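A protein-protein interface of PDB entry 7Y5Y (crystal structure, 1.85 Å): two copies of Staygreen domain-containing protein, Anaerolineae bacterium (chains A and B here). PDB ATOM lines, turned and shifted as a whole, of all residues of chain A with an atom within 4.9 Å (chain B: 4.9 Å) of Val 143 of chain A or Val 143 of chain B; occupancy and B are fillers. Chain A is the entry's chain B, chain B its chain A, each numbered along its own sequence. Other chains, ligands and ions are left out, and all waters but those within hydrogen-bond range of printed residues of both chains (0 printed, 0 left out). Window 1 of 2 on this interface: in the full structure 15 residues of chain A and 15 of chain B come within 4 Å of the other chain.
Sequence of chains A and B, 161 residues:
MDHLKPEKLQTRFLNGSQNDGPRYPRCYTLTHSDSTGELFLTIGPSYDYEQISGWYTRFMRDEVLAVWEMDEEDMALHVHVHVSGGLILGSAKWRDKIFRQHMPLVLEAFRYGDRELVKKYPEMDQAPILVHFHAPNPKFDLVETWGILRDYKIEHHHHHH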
ATOM      1  N   LEU A 130       1.551  22.495   9.892  1.00  0.00           N
ATOM      2  CA  LEU A 130       2.562  21.795   9.113  1.00  0.00           C
ATOM      3  C   LEU A 130       3.904  22.477   9.336  1.00  0.00           C
ATOM      4  O   LEU A 130       4.027  23.680   9.101  1.00  0.00           O
ATOM      5  CB  LEU A 130       2.205  21.819   7.630  1.00  0.00           C
ATOM      6  CG  LEU A 130       1.354  20.669   7.106  1.00  0.00           C
ATOM      7  CD1 LEU A 130       1.042  20.928   5.651  1.00  0.00           C
ATOM      8  CD2 LEU A 130       2.074  19.339   7.254  1.00  0.00           C
ATOM      9  N   VAL A 131       4.906  21.713   9.773  1.00  0.00           N
ATOM     10  CA  VAL A 131       6.248  22.238  10.025  1.00  0.00           C
ATOM     11  C   VAL A 131       7.187  21.689   8.963  1.00  0.00           C
ATOM     12  O   VAL A 131       7.315  20.465   8.797  1.00  0.00           O
ATOM     13  CB  VAL A 131       6.740  21.889  11.442  1.00  0.00           C
ATOM     14  CG1 VAL A 131       8.122  22.519  11.699  1.00  0.00           C
ATOM     15  CG2 VAL A 131       5.730  22.392  12.473  1.00  0.00           C
ATOM     16  N   HIS A 132       7.865  22.591   8.254  1.00  0.00           N
ATOM     17  CA  HIS A 132       8.899  22.235   7.290  1.00  0.00           C
ATOM     18  C   HIS A 132      10.257  22.573   7.900  1.00  0.00           C
ATOM     19  O   HIS A 132      10.559  23.750   8.133  1.00  0.00           O
ATOM     20  CB  HIS A 132       8.694  22.967   5.965  1.00  0.00           C
ATOM     21  CG  HIS A 132       9.537  22.454   4.842  1.00  0.00           C
ATOM     22  ND1 HIS A 132       9.264  22.753   3.521  1.00  0.00           N
ATOM     23  CD2 HIS A 132      10.684  21.724   4.835  1.00  0.00           C
ATOM     24  CE1 HIS A 132      10.178  22.195   2.749  1.00  0.00           C
ATOM     25  NE2 HIS A 132      11.052  21.564   3.523  1.00  0.00           N
ATOM     26  N   ASP A 141      15.497  17.392   5.539  1.00  0.00           N
ATOM     27  CA  ASP A 141      14.434  18.129   4.855  1.00  0.00           C
ATOM     28  C   ASP A 141      13.062  17.472   4.988  1.00  0.00           C
ATOM     29  O   ASP A 141      12.647  16.708   4.114  1.00  0.00           O
ATOM     30  CB  ASP A 141      14.833  18.314   3.391  1.00  0.00           C
ATOM     31  CG  ASP A 141      14.018  19.418   2.694  1.00  0.00           C
ATOM     32  OD1 ASP A 141      13.592  20.367   3.373  1.00  0.00           O
ATOM     33  OD2 ASP A 141      13.899  19.362   1.452  1.00  0.00           O
ATOM     34  N   LEU A 142      12.350  17.781   6.065  1.00  0.00           N
ATOM     35  CA  LEU A 142      11.141  17.054   6.432  1.00  0.00           C
ATOM     36  C   LEU A 142       9.968  17.999   6.639  1.00  0.00           C
ATOM     37  O   LEU A 142      10.111  19.080   7.216  1.00  0.00           O
ATOM     38  CB  LEU A 142      11.354  16.243   7.718  1.00  0.00           C
ATOM     39  CG  LEU A 142      12.500  15.218   7.627  1.00  0.00           C
ATOM     40  CD1 LEU A 142      12.727  14.553   8.977  1.00  0.00           C
ATOM     41  CD2 LEU A 142      12.297  14.189   6.520  1.00  0.00           C
ATOM     42  N   VAL A 143       8.795  17.555   6.207  1.00  0.00           N
ATOM     43  CA  VAL A 143       7.541  18.260   6.426  1.00  0.00           C
ATOM     44  C   VAL A 143       6.690  17.392   7.338  1.00  0.00           C
ATOM     45  O   VAL A 143       6.444  16.221   7.025  1.00  0.00           O
ATOM     46  CB  VAL A 143       6.826  18.550   5.100  1.00  0.00           C
ATOM     47  CG1 VAL A 143       5.435  19.062   5.374  1.00  0.00           C
ATOM     48  CG2 VAL A 143       7.624  19.565   4.310  1.00  0.00           C
ATOM     49  N   GLU A 144       6.259  17.947   8.473  1.00  0.00           N
ATOM     50  CA  GLU A 144       5.602  17.156   9.509  1.00  0.00           C
ATOM     51  C   GLU A 144       4.363  17.839  10.050  1.00  0.00           C
ATOM     52  O   GLU A 144       4.334  19.059  10.241  1.00  0.00           O
ATOM     53  CB  GLU A 144       6.568  16.858  10.686  1.00  0.00           C
ATOM     54  CG  GLU A 144       7.817  16.145  10.267  1.00  0.00           C
ATOM     55  CD  GLU A 144       8.818  15.974  11.425  1.00  0.00           C
ATOM     56  OE1 GLU A 144       8.551  16.485  12.529  1.00  0.00           O
ATOM     57  OE2 GLU A 144       9.856  15.314  11.224  1.00  0.00           O
ATOM     58  N   THR A 145       3.342  17.034  10.330  1.00  0.00           N
ATOM     59  CA  THR A 145       2.169  17.545  11.007  1.00  0.00           C
ATOM     60  C   THR A 145       2.422  17.559  12.510  1.00  0.00           C
ATOM     61  O   THR A 145       2.836  16.554  13.095  1.00  0.00           O
ATOM     62  CB  THR A 145       0.934  16.712  10.656  1.00  0.00           C
ATOM     63  OG1 THR A 145       0.780  16.691   9.228  1.00  0.00           O
ATOM     64  CG2 THR A 145      -0.295  17.329  11.261  1.00  0.00           C
ATOM     65  N   LEU B 130      15.136  15.191  -4.735  1.00  0.00           N
ATOM     66  CA  LEU B 130      14.143  15.314  -3.693  1.00  0.00           C
ATOM     67  C   LEU B 130      12.967  16.086  -4.294  1.00  0.00           C
ATOM     68  O   LEU B 130      13.174  17.166  -4.852  1.00  0.00           O
ATOM     69  CB  LEU B 130      14.783  15.997  -2.494  1.00  0.00           C
ATOM     70  CG  LEU B 130      14.039  16.169  -1.190  1.00  0.00           C
ATOM     71  CD1 LEU B 130      13.817  14.686  -0.815  1.00  0.00           C
ATOM     72  CD2 LEU B 130      14.951  16.781  -0.160  1.00  0.00           C
ATOM     73  N   VAL B 131      11.763  15.499  -4.290  1.00  0.00           N
ATOM     74  CA  VAL B 131      10.607  16.109  -4.966  1.00  0.00           C
ATOM     75  C   VAL B 131       9.636  16.610  -3.914  1.00  0.00           C
ATOM     76  O   VAL B 131       9.197  15.849  -3.043  1.00  0.00           O
ATOM     77  CB  VAL B 131       9.905  15.141  -5.945  1.00  0.00           C
ATOM     78  CG1 VAL B 131       8.761  15.879  -6.696  1.00  0.00           C
ATOM     79  CG2 VAL B 131      10.881  14.586  -6.949  1.00  0.00           C
ATOM     80  N   HIS B 132       9.294  17.900  -3.990  1.00  0.00           N
ATOM     81  CA  HIS B 132       8.318  18.483  -3.088  1.00  0.00           C
ATOM     82  C   HIS B 132       7.028  18.668  -3.869  1.00  0.00           C
ATOM     83  O   HIS B 132       6.990  19.458  -4.814  1.00  0.00           O
ATOM     84  CB  HIS B 132       8.800  19.812  -2.514  1.00  0.00           C
ATOM     85  CG  HIS B 132       7.928  20.360  -1.432  1.00  0.00           C
ATOM     86  ND1 HIS B 132       8.370  21.316  -0.547  1.00  0.00           N
ATOM     87  CD2 HIS B 132       6.626  20.132  -1.121  1.00  0.00           C
ATOM     88  CE1 HIS B 132       7.394  21.628   0.285  1.00  0.00           C
ATOM     89  NE2 HIS B 132       6.322  20.923  -0.041  1.00  0.00           N
ATOM     90  N   ASP B 141       0.824  17.637   0.669  1.00  0.00           N
ATOM     91  CA  ASP B 141       2.072  18.386   0.824  1.00  0.00           C
ATOM     92  C   ASP B 141       3.166  17.457   1.327  1.00  0.00           C
ATOM     93  O   ASP B 141       3.376  17.319   2.528  1.00  0.00           O
ATOM     94  CB  ASP B 141       1.871  19.555   1.773  1.00  0.00           C
ATOM     95  CG  ASP B 141       3.040  20.544   1.736  1.00  0.00           C
ATOM     96  OD1 ASP B 141       3.670  20.679   0.666  1.00  0.00           O
ATOM     97  OD2 ASP B 141       3.258  21.231   2.757  1.00  0.00           O
ATOM     98  N   LEU B 142       3.896  16.848   0.390  1.00  0.00           N
ATOM     99  CA  LEU B 142       4.850  15.793   0.716  1.00  0.00           C
ATOM    100  C   LEU B 142       6.190  16.039   0.041  1.00  0.00           C
ATOM    101  O   LEU B 142       6.248  16.420  -1.130  1.00  0.00           O
ATOM    102  CB  LEU B 142       4.330  14.414   0.277  1.00  0.00           C
ATOM    103  CG  LEU B 142       2.956  14.010   0.823  1.00  0.00           C
ATOM    104  CD1 LEU B 142       2.471  12.783   0.075  1.00  0.00           C
ATOM    105  CD2 LEU B 142       2.987  13.768   2.327  1.00  0.00           C
ATOM    106  N   VAL B 143       7.271  15.770   0.775  1.00  0.00           N
ATOM    107  CA  VAL B 143       8.634  15.792   0.249  1.00  0.00           C
ATOM    108  C   VAL B 143       9.143  14.358   0.200  1.00  0.00           C
ATOM    109  O   VAL B 143       9.103  13.651   1.216  1.00  0.00           O
ATOM    110  CB  VAL B 143       9.556  16.664   1.118  1.00  0.00           C
ATOM    111  CG1 VAL B 143      11.021  16.553   0.627  1.00  0.00           C
ATOM    112  CG2 VAL B 143       9.079  18.100   1.122  1.00  0.00           C
ATOM    113  N   GLU B 144       9.597  13.926  -0.974  1.00  0.00           N
ATOM    114  CA  GLU B 144       9.959  12.531  -1.220  1.00  0.00           C
ATOM    115  C   GLU B 144      11.268  12.412  -1.984  1.00  0.00           C
ATOM    116  O   GLU B 144      11.519  13.148  -2.944  1.00  0.00           O
ATOM    117  CB  GLU B 144       8.853  11.774  -2.009  1.00  0.00           C
ATOM    118  CG  GLU B 144       7.470  11.910  -1.414  1.00  0.00           C
ATOM    119  CD  GLU B 144       6.366  11.195  -2.224  1.00  0.00           C
ATOM    120  OE1 GLU B 144       6.611  10.787  -3.376  1.00  0.00           O
ATOM    121  OE2 GLU B 144       5.247  11.054  -1.681  1.00  0.00           O
ATOM    122  N   THR B 145      12.090  11.442  -1.587  1.00  0.00           N
ATOM    123  CA  THR B 145      13.256  11.121  -2.385  1.00  0.00           C
ATOM    124  C   THR B 145      12.858  10.239  -3.558  1.00  0.00           C
ATOM    125  O   THR B 145      12.172   9.228  -3.383  1.00  0.00           O
ATOM    126  CB  THR B 145      14.333  10.450  -1.527  1.00  0.00           C
ATOM    127  OG1 THR B 145      14.490  11.180  -0.300  1.00  0.00           O
ATOM    128  CG2 THR B 145      15.636  10.427  -2.268  1.00  0.00           C
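Of chain A, only Asp 141 and Val 143 come within 4 Å of Val 143 of chain B.
Of the printed residues of chain A, Leu 130 of chain B touches Asp 141.
Of the printed residues of chain B, His 132 of chain A touches His 132.
Thr 145 of chain B touches none of the printed residues of chain A.
Val 131 of chain B touches none of the printed residues of chain A.
Of the 8 printed residues of chain B, 4 touch a printed residue of chain A.
Hydrophobic or aromatic side chains of chain B that line the printed part of chain A: Leu 130, His 132 and Val 143.
Of the 8 printed residues of chain A, 4 touch a printed residue of chain B.
Among the printed residues, 6 pairs touch across the chains.
Among the printed residues, merely in contact across the chains: Leu 130 of chain A with Asp 141 of chain B, His 132 of chain A with His 132 of chain B, Asp 141 of chain A with Leu 130 of chain B, Asp 141 of chain A with Val 143 of chain B, Val 143 of chain A with Asp 141 of chain B and Val 143 of chain A with Val 143 of chain B.
Leu 130 of chain A touches Asp 141 of chain B, and with the chains exchanged Asp 141 of chain A touches Leu 130 of chain B.
His 132 of chain A touches its own counterpart, His 132 of chain B.
Asp 141 of chain A touches Val 143 of chain B, and with the chains exchanged Val 143 of chain A touches Asp 141 of chain B.
Val 143 of chain B touches its own counterpart, Val 143 of chain A.
A ring nitrogen (NE2) of His 132 of chain B is in hydrogen-bond range of the side-chain carboxylate (OD1) of Asp 141 of chain B.
NE2 of His 132 of chain A sits at hydrogen-bond distance from OD1 of Asp 141 of chain A (2.8 Å).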
